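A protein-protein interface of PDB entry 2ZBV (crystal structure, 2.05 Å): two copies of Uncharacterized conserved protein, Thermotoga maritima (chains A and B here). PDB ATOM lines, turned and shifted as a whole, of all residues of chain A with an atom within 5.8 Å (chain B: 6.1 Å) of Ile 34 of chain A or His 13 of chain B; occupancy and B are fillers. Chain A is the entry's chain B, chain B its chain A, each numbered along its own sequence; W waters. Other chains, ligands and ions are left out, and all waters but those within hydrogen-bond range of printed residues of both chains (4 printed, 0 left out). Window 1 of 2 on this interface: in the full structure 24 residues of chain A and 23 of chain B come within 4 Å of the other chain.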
ATOM      1  N   GLY A   3      17.801 -27.057  -7.242  1.00  0.00           N
ATOM      2  CA  GLY A   3      16.769 -27.062  -8.267  1.00  0.00           C
ATOM      3  C   GLY A   3      15.578 -27.783  -7.658  1.00  0.00           C
ATOM      4  O   GLY A   3      15.688 -28.953  -7.300  1.00  0.00           O
ATOM      5  N   PHE A   4      14.440 -27.100  -7.563  1.00  0.00           N
ATOM      6  CA  PHE A   4      13.237 -27.643  -6.930  1.00  0.00           C
ATOM      7  C   PHE A   4      12.145 -28.066  -7.944  1.00  0.00           C
ATOM      8  O   PHE A   4      11.638 -27.238  -8.704  1.00  0.00           O
ATOM      9  CB  PHE A   4      12.719 -26.560  -5.968  1.00  0.00           C
ATOM     10  CG  PHE A   4      11.823 -27.059  -4.863  1.00  0.00           C
ATOM     11  CD1 PHE A   4      11.576 -28.416  -4.672  1.00  0.00           C
ATOM     12  CD2 PHE A   4      11.218 -26.140  -4.000  1.00  0.00           C
ATOM     13  CE1 PHE A   4      10.732 -28.854  -3.629  1.00  0.00           C
ATOM     14  CE2 PHE A   4      10.380 -26.563  -2.965  1.00  0.00           C
ATOM     15  CZ  PHE A   4      10.137 -27.924  -2.778  1.00  0.00           C
ATOM     16  N   LEU A   5      11.783 -29.350  -7.927  1.00  0.00           N
ATOM     17  CA  LEU A   5      10.781 -29.914  -8.844  1.00  0.00           C
ATOM     18  C   LEU A   5       9.781 -30.828  -8.134  1.00  0.00           C
ATOM     19  O   LEU A   5      10.166 -31.788  -7.462  1.00  0.00           O
ATOM     20  CB  LEU A   5      11.492 -30.694  -9.961  1.00  0.00           C
ATOM     21  CG  LEU A   5      10.700 -31.586 -10.929  1.00  0.00           C
ATOM     22  CD1 LEU A   5       9.559 -30.811 -11.548  1.00  0.00           C
ATOM     23  CD2 LEU A   5      11.636 -32.101 -12.025  1.00  0.00           C
ATOM     24  N   ILE A  32      15.936 -22.472  -6.674  1.00  0.00           N
ATOM     25  CA  ILE A  32      15.390 -22.161  -7.985  1.00  0.00           C
ATOM     26  C   ILE A  32      14.341 -23.199  -8.358  1.00  0.00           C
ATOM     27  O   ILE A  32      14.635 -24.389  -8.471  1.00  0.00           O
ATOM     28  CB  ILE A  32      16.482 -22.140  -9.077  1.00  0.00           C
ATOM     29  CG1 ILE A  32      17.545 -21.099  -8.716  1.00  0.00           C
ATOM     30  CG2 ILE A  32      15.854 -21.802 -10.443  1.00  0.00           C
ATOM     31  CD1 ILE A  32      18.552 -20.848  -9.803  1.00  0.00           C
ATOM     32  N   ASP A  33      13.108 -22.738  -8.523  1.00  0.00           N
ATOM     33  CA  ASP A  33      11.998 -23.609  -8.889  1.00  0.00           C
ATOM     34  C   ASP A  33      12.097 -24.026 -10.344  1.00  0.00           C
ATOM     35  O   ASP A  33      12.163 -23.178 -11.232  1.00  0.00           O
ATOM     36  CB  ASP A  33      10.676 -22.878  -8.673  1.00  0.00           C
ATOM     37  CG  ASP A  33      10.420 -22.559  -7.214  1.00  0.00           C
ATOM     38  OD1 ASP A  33       9.811 -21.508  -6.938  1.00  0.00           O
ATOM     39  OD2 ASP A  33      10.817 -23.367  -6.346  1.00  0.00           O
ATOM     40  N   ILE A  34      12.125 -25.327 -10.594  1.00  0.00           N
ATOM     41  CA  ILE A  34      12.171 -25.818 -11.967  1.00  0.00           C
ATOM     42  C   ILE A  34      10.694 -25.762 -12.392  1.00  0.00           C
ATOM     43  O   ILE A  34      10.340 -25.122 -13.385  1.00  0.00           O
ATOM     44  CB  ILE A  34      12.752 -27.249 -12.010  1.00  0.00           C
ATOM     45  CG1 ILE A  34      14.248 -27.185 -11.661  1.00  0.00           C
ATOM     46  CG2 ILE A  34      12.551 -27.870 -13.391  1.00  0.00           C
ATOM     47  CD1 ILE A  34      14.970 -28.516 -11.715  1.00  0.00           C
ATOM     48  N   THR A  35       9.851 -26.428 -11.608  1.00  0.00           N
ATOM     49  CA  THR A  35       8.399 -26.412 -11.780  1.00  0.00           C
ATOM     50  C   THR A  35       7.732 -27.185 -10.658  1.00  0.00           C
ATOM     51  O   THR A  35       8.308 -28.129 -10.107  1.00  0.00           O
ATOM     52  CB  THR A  35       7.905 -27.001 -13.119  1.00  0.00           C
ATOM     53  OG1 THR A  35       6.476 -26.852 -13.189  1.00  0.00           O
ATOM     54  CG2 THR A  35       8.236 -28.474 -13.234  1.00  0.00           C
ATOM     55  N   HIS A  36       6.523 -26.757 -10.306  1.00  0.00           N
ATOM     56  CA  HIS A  36       5.746 -27.422  -9.275  1.00  0.00           C
ATOM     57  C   HIS A  36       4.407 -27.800  -9.889  1.00  0.00           C
ATOM     58  O   HIS A  36       3.470 -28.166  -9.185  1.00  0.00           O
ATOM     59  CB  HIS A  36       5.554 -26.485  -8.076  1.00  0.00           C
ATOM     60  CG  HIS A  36       6.819 -26.222  -7.319  1.00  0.00           C
ATOM     61  ND1 HIS A  36       7.447 -27.194  -6.571  1.00  0.00           N
ATOM     62  CD2 HIS A  36       7.616 -25.128  -7.260  1.00  0.00           C
ATOM     63  CE1 HIS A  36       8.579 -26.712  -6.087  1.00  0.00           C
ATOM     64  NE2 HIS A  36       8.706 -25.461  -6.490  1.00  0.00           N
ATOM     65  N   VAL A  49      11.369 -33.635 -17.529  1.00  0.00           N
ATOM     66  CA  VAL A  49      11.538 -32.220 -17.196  1.00  0.00           C
ATOM     67  C   VAL A  49      12.826 -32.025 -16.403  1.00  0.00           C
ATOM     68  O   VAL A  49      13.575 -31.098 -16.660  1.00  0.00           O
ATOM     69  CB  VAL A  49      10.344 -31.669 -16.380  1.00  0.00           C
ATOM     70  CG1 VAL A  49      10.668 -30.277 -15.853  1.00  0.00           C
ATOM     71  CG2 VAL A  49       9.098 -31.592 -17.270  1.00  0.00           C
ATOM     72  N   LEU A  50      13.069 -32.912 -15.441  1.00  0.00           N
ATOM     73  CA  LEU A  50      14.268 -32.855 -14.612  1.00  0.00           C
ATOM     74  C   LEU A  50      15.527 -32.839 -15.479  1.00  0.00           C
ATOM     75  O   LEU A  50      16.402 -31.987 -15.313  1.00  0.00           O
ATOM     76  CB  LEU A  50      14.313 -34.067 -13.674  1.00  0.00           C
ATOM     77  CG  LEU A  50      15.572 -34.208 -12.812  1.00  0.00           C
ATOM     78  CD1 LEU A  50      15.713 -32.970 -11.931  1.00  0.00           C
ATOM     79  CD2 LEU A  50      15.489 -35.475 -11.953  1.00  0.00           C
ATOM     80  N   ARG A  52      15.901 -32.185 -18.811  1.00  0.00           N
ATOM     81  CA  ARG A  52      16.014 -31.021 -19.674  1.00  0.00           C
ATOM     82  C   ARG A  52      16.405 -29.767 -18.922  1.00  0.00           C
ATOM     83  O   ARG A  52      17.201 -28.968 -19.422  1.00  0.00           O
ATOM     84  CB  ARG A  52      14.716 -30.837 -20.459  1.00  0.00           C
ATOM     85  CG  ARG A  52      14.463 -32.080 -21.301  1.00  0.00           C
ATOM     86  CD  ARG A  52      13.212 -32.053 -22.128  1.00  0.00           C
ATOM     87  NE  ARG A  52      13.042 -33.347 -22.787  1.00  0.00           N
ATOM     88  CZ  ARG A  52      12.419 -33.522 -23.947  1.00  0.00           C
ATOM     89  NH1 ARG A  52      11.903 -32.482 -24.585  1.00  0.00           N
ATOM     90  NH2 ARG A  52      12.318 -34.737 -24.470  1.00  0.00           N
ATOM     91  N   ALA A  53      15.883 -29.597 -17.711  1.00  0.00           N
ATOM     92  CA  ALA A  53      16.235 -28.419 -16.929  1.00  0.00           C
ATOM     93  C   ALA A  53      17.670 -28.519 -16.395  1.00  0.00           C
ATOM     94  O   ALA A  53      18.404 -27.527 -16.387  1.00  0.00           O
ATOM     95  CB  ALA A  53      15.268 -28.248 -15.773  1.00  0.00           C
ATOM     96  N   SER A  54      18.058 -29.718 -15.958  1.00  0.00           N
ATOM     97  CA  SER A  54      19.393 -29.953 -15.395  1.00  0.00           C
ATOM     98  C   SER A  54      20.541 -29.602 -16.339  1.00  0.00           C
ATOM     99  O   SER A  54      21.660 -29.350 -15.888  1.00  0.00           O
ATOM    100  CB  SER A  54      19.538 -31.415 -14.945  1.00  0.00           C
ATOM    101  OG  SER A  54      19.552 -32.299 -16.054  1.00  0.00           O
ATOM    102  N   PHE A  57      21.775 -26.122 -15.463  1.00  0.00           N
ATOM    103  CA  PHE A  57      22.203 -25.880 -14.092  1.00  0.00           C
ATOM    104  C   PHE A  57      23.671 -26.289 -14.033  1.00  0.00           C
ATOM    105  O   PHE A  57      24.092 -27.223 -14.712  1.00  0.00           O
ATOM    106  CB  PHE A  57      21.384 -26.728 -13.120  1.00  0.00           C
ATOM    107  CG  PHE A  57      20.095 -26.088 -12.694  1.00  0.00           C
ATOM    108  CD1 PHE A  57      20.009 -25.414 -11.476  1.00  0.00           C
ATOM    109  CD2 PHE A  57      18.963 -26.172 -13.493  1.00  0.00           C
ATOM    110  CE1 PHE A  57      18.812 -24.838 -11.059  1.00  0.00           C
ATOM    111  CE2 PHE A  57      17.755 -25.596 -13.086  1.00  0.00           C
ATOM    112  CZ  PHE A  57      17.682 -24.928 -11.862  1.00  0.00           C
ATOM    113  N   PHE A  63      19.516 -31.196  -6.700  1.00  0.00           N
ATOM    114  CA  PHE A  63      18.128 -31.197  -7.143  1.00  0.00           C
ATOM    115  C   PHE A  63      17.212 -31.875  -6.141  1.00  0.00           C
ATOM    116  O   PHE A  63      17.458 -33.007  -5.727  1.00  0.00           O
ATOM    117  CB  PHE A  63      18.012 -31.904  -8.492  1.00  0.00           C
ATOM    118  CG  PHE A  63      18.677 -31.171  -9.617  1.00  0.00           C
ATOM    119  CD1 PHE A  63      17.980 -30.213 -10.344  1.00  0.00           C
ATOM    120  CD2 PHE A  63      20.000 -31.439  -9.953  1.00  0.00           C
ATOM    121  CE1 PHE A  63      18.593 -29.532 -11.399  1.00  0.00           C
ATOM    122  CE2 PHE A  63      20.620 -30.767 -11.002  1.00  0.00           C
ATOM    123  CZ  PHE A  63      19.915 -29.811 -11.728  1.00  0.00           C
ATOM    124  N   ILE A 176       7.096 -33.754 -23.793  1.00  0.00           N
ATOM    125  CA  ILE A 176       6.519 -32.609 -23.109  1.00  0.00           C
ATOM    126  C   ILE A 176       5.778 -31.646 -24.029  1.00  0.00           C
ATOM    127  O   ILE A 176       6.216 -31.358 -25.143  1.00  0.00           O
ATOM    128  CB  ILE A 176       7.614 -31.806 -22.382  1.00  0.00           C
ATOM    129  CG1 ILE A 176       8.347 -32.710 -21.388  1.00  0.00           C
ATOM    130  CG2 ILE A 176       6.997 -30.604 -21.672  1.00  0.00           C
ATOM    131  CD1 ILE A 176       9.586 -32.076 -20.787  1.00  0.00           C
ATOM    132  N   SER A 234      15.124 -25.789 -27.219  1.00  0.00           N
ATOM    133  CA  SER A 234      16.259 -25.300 -26.435  1.00  0.00           C
ATOM    134  C   SER A 234      17.081 -26.350 -25.697  1.00  0.00           C
ATOM    135  O   SER A 234      18.069 -26.013 -25.038  1.00  0.00           O
ATOM    136  CB  SER A 234      15.784 -24.252 -25.436  1.00  0.00           C
ATOM    137  OG  SER A 234      14.921 -24.829 -24.480  1.00  0.00           O
ATOM    138  N   ALA A 235      16.677 -27.611 -25.792  1.00  0.00           N
ATOM    139  CA  ALA A 235      17.412 -28.686 -25.137  1.00  0.00           C
ATOM    140  C   ALA A 235      18.010 -29.625 -26.189  1.00  0.00           C
ATOM    141  O   ALA A 235      18.703 -30.582 -25.857  1.00  0.00           O
ATOM    142  CB  ALA A 235      16.490 -29.458 -24.190  1.00  0.00           C
ATOM    143  N   GLY B   9       5.117 -18.878 -18.768  1.00  0.00           N
ATOM    144  CA  GLY B   9       4.304 -19.688 -17.869  1.00  0.00           C
ATOM    145  C   GLY B   9       5.162 -20.268 -16.754  1.00  0.00           C
ATOM    146  O   GLY B   9       6.356 -20.463 -16.933  1.00  0.00           O
ATOM    147  N   LEU B  10       4.562 -20.546 -15.601  1.00  0.00           N
ATOM    148  CA  LEU B  10       5.303 -21.106 -14.473  1.00  0.00           C
ATOM    149  C   LEU B  10       5.258 -22.629 -14.479  1.00  0.00           C
ATOM    150  O   LEU B  10       5.926 -23.289 -13.678  1.00  0.00           O
ATOM    151  CB  LEU B  10       4.743 -20.576 -13.148  1.00  0.00           C
ATOM    152  CG  LEU B  10       5.086 -19.123 -12.794  1.00  0.00           C
ATOM    153  CD1 LEU B  10       4.406 -18.738 -11.487  1.00  0.00           C
ATOM    154  CD2 LEU B  10       6.596 -18.957 -12.675  1.00  0.00           C
ATOM    155  N   LYS B  11       4.474 -23.185 -15.391  1.00  0.00           N
ATOM    156  CA  LYS B  11       4.347 -24.630 -15.506  1.00  0.00           C
ATOM    157  C   LYS B  11       5.586 -25.265 -16.144  1.00  0.00           C
ATOM    158  O   LYS B  11       6.015 -26.349 -15.744  1.00  0.00           O
ATOM    159  CB  LYS B  11       3.091 -24.980 -16.313  1.00  0.00           C
ATOM    160  CG  LYS B  11       2.925 -26.464 -16.580  1.00  0.00           C
ATOM    161  CD  LYS B  11       1.550 -26.791 -17.140  1.00  0.00           C
ATOM    162  CE  LYS B  11       1.466 -28.265 -17.527  1.00  0.00           C
ATOM    163  NZ  LYS B  11       1.869 -29.167 -16.404  1.00  0.00           N
ATOM    164  N   SER B  12       6.164 -24.596 -17.135  1.00  0.00           N
ATOM    165  CA  SER B  12       7.359 -25.124 -17.792  1.00  0.00           C
ATOM    166  C   SER B  12       8.604 -24.794 -16.969  1.00  0.00           C
ATOM    167  O   SER B  12       8.546 -23.999 -16.028  1.00  0.00           O
ATOM    168  CB  SER B  12       7.505 -24.532 -19.199  1.00  0.00           C
ATOM    169  OG  SER B  12       6.430 -24.934 -20.032  1.00  0.00           O
ATOM    170  N   HIS B  13       9.726 -25.403 -17.337  1.00  0.00           N
ATOM    171  CA  HIS B  13      10.995 -25.182 -16.649  1.00  0.00           C
ATOM    172  C   HIS B  13      11.779 -24.007 -17.239  1.00  0.00           C
ATOM    173  O   HIS B  13      12.887 -23.702 -16.790  1.00  0.00           O
ATOM    174  CB  HIS B  13      11.860 -26.447 -16.730  1.00  0.00           C
ATOM    175  CG  HIS B  13      12.264 -26.813 -18.125  1.00  0.00           C
ATOM    176  ND1 HIS B  13      11.460 -27.556 -18.962  1.00  0.00           N
ATOM    177  CD2 HIS B  13      13.368 -26.500 -18.843  1.00  0.00           C
ATOM    178  CE1 HIS B  13      12.051 -27.687 -20.138  1.00  0.00           C
ATOM    179  NE2 HIS B  13      13.210 -27.054 -20.092  1.00  0.00           N
ATOM    180  N   TYR B  14      11.206 -23.340 -18.235  1.00  0.00           N
ATOM    181  CA  TYR B  14      11.890 -22.228 -18.884  1.00  0.00           C
ATOM    182  C   TYR B  14      12.285 -21.111 -17.935  1.00  0.00           C
ATOM    183  O   TYR B  14      13.420 -20.634 -17.958  1.00  0.00           O
ATOM    184  CB  TYR B  14      11.020 -21.648 -20.004  1.00  0.00           C
ATOM    185  CG  TYR B  14      10.561 -22.671 -21.026  1.00  0.00           C
ATOM    186  CD1 TYR B  14      11.442 -23.630 -21.521  1.00  0.00           C
ATOM    187  CD2 TYR B  14       9.258 -22.646 -21.526  1.00  0.00           C
ATOM    188  CE1 TYR B  14      11.040 -24.542 -22.496  1.00  0.00           C
ATOM    189  CE2 TYR B  14       8.841 -23.552 -22.505  1.00  0.00           C
ATOM    190  CZ  TYR B  14       9.738 -24.497 -22.987  1.00  0.00           C
ATOM    191  OH  TYR B  14       9.336 -25.392 -23.961  1.00  0.00           O
ATOM    192  N   VAL B  15      11.352 -20.680 -17.101  1.00  0.00           N
ATOM    193  CA  VAL B  15      11.661 -19.605 -16.177  1.00  0.00           C
ATOM    194  C   VAL B  15      12.818 -20.001 -15.266  1.00  0.00           C
ATOM    195  O   VAL B  15      13.756 -19.230 -15.077  1.00  0.00           O
ATOM    196  CB  VAL B  15      10.432 -19.232 -15.329  1.00  0.00           C
ATOM    197  CG1 VAL B  15      10.847 -18.321 -14.188  1.00  0.00           C
ATOM    198  CG2 VAL B  15       9.400 -18.536 -16.217  1.00  0.00           C
ATOM    199  N   GLY B  16      12.754 -21.212 -14.721  1.00  0.00           N
ATOM    200  CA  GLY B  16      13.811 -21.678 -13.838  1.00  0.00           C
ATOM    201  C   GLY B  16      15.196 -21.733 -14.467  1.00  0.00           C
ATOM    202  O   GLY B  16      16.176 -21.359 -13.821  1.00  0.00           O
ATOM    203  N   VAL B  17      15.303 -22.195 -15.714  1.00  0.00           N
ATOM    204  CA  VAL B  17      16.625 -22.273 -16.344  1.00  0.00           C
ATOM    205  C   VAL B  17      17.212 -20.895 -16.605  1.00  0.00           C
ATOM    206  O   VAL B  17      18.420 -20.717 -16.526  1.00  0.00           O
ATOM    207  CB  VAL B  17      16.606 -23.095 -17.667  1.00  0.00           C
ATOM    208  CG1 VAL B  17      16.260 -24.539 -17.369  1.00  0.00           C
ATOM    209  CG2 VAL B  17      15.612 -22.515 -18.647  1.00  0.00           C
ATOM    210  N   ALA B  18      16.356 -19.923 -16.919  1.00  0.00           N
ATOM    211  CA  ALA B  18      16.808 -18.558 -17.151  1.00  0.00           C
ATOM    212  C   ALA B  18      17.324 -17.985 -15.835  1.00  0.00           C
ATOM    213  O   ALA B  18      18.311 -17.244 -15.814  1.00  0.00           O
ATOM    214  CB  ALA B  18      15.673 -17.697 -17.673  1.00  0.00           C
HETATM  215  O   HOH W   1      15.323 -26.646 -22.419  1.00  0.00           O
HETATM  216  O   HOH W   2       8.353 -22.532 -12.729  1.00  0.00           O
HETATM  217  O   HOH W   3       5.450 -24.149 -11.126  1.00  0.00           O
HETATM  218  O   HOH W   4      10.306 -22.611 -14.485  1.00  0.00           O
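N of Phe 4 of chain A is in hydrogen-bond range of O of Ile 32 of chain A.
The backbone NH of Ile 34 of chain A lies within hydrogen-bond range of the backbone carbonyl oxygen of Phe 4 of chain A.
A ring nitrogen (NE2) of His 36 of chain A is in hydrogen-bond range of the side-chain carboxylate of Asp 33 of chain A, at 3.0 Å.
Water W2 lies within hydrogen-bond range of O of Leu 10 of chain B (2.7 Å) and O of Ile 34 of chain A (3.3 Å).
Water W4 lies within hydrogen-bond range of the backbone carbonyl oxygen of Ser 12 of chain B (2.7 Å), the backbone carbonyl oxygen of Ile 34 of chain A (2.7 Å), the backbone NH of Gly 16 of chain B (2.8 Å) and the backbone NH of Val 15 of chain B (3.4 Å).
Water W3 bridges the backbone carbonyl oxygen (O) of Leu 10 of chain B (2.7 Å) and the backbone NH (N) of His 36 of chain A (2.9 Å).
Water W1 bridges OG of Ser 234 of chain A (2.8 Å) and NE2 of His 13 of chain B (3.2 Å).
O of Lys 11 of chain B sits at hydrogen-bond distance from OG1 of Thr 35 of chain A, 2.6 Å away.
O of Ile 34 of chain A sits close to O of Ser 12 of chain B (3.4 Å).
Of the 18 printed residues of chain A, 5 touch a printed residue of chain B.
Printed residues of chain A that touch a printed residue of chain B: Ile 32, Asp 33, Ile 34, Thr 35 and Ala 53.
Hydrophobic or aromatic side chains of chain A that line the printed part of chain B: Ile 32, Ile 34 and Ala 53.
Hydrophobic or aromatic side chains of chain B that line the printed part of chain A: His 13 and Val 17.
Among the printed residues, 8 pairs touch across the chains.
Among the printed residues, pairs that only touch across the chains: Ile 32 of chain A with Gly 16 of chain B (3.4 Å), Asp 33 of chain A with Gly 16 of chain B (3.4 Å), Ile 34 of chain A with His 13 of chain B (3.3 Å), Thr 35 of chain A with Leu 10 of chain B (3.6 Å), Ala 53 of chain A with His 13 of chain B (3.9 Å) and Ala 53 of chain A with Val 17 of chain B (3.8 Å).
Printed residues of chain B within 4 Å of Ile 34 of chain A: Ser 12 (3.4 Å) and His 13 (3.3 Å).
Of the printed residues of chain A, Leu 10 of chain B touches Thr 35 (3.6 Å).
Printed residues of chain A within 4 Å of Lys 11 of chain B: Thr 35 (2.6 Å).
Of chain A, only Ile 34 and Ala 53 come within 4 Å of His 13 of chain B.
Val 15 of chain B touches none of the printed residues of chain A.
Printed residues of chain A within 4 Å of Gly 16 of chain B: Ile 32 (3.4 Å) and Asp 33 (3.4 Å).
Of the printed residues of chain A, Val 17 of chain B touches Ala 53 (3.8 Å).
The nearest printed residue of chain B that does not touch Ile 34 of chain A is Gly 16 of chain B (4.8 Å).
The nearest printed residue of chain A that does not touch Lys 11 of chain B is Ile 34 of chain A (5.1 Å).
No position is printed for both chains.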
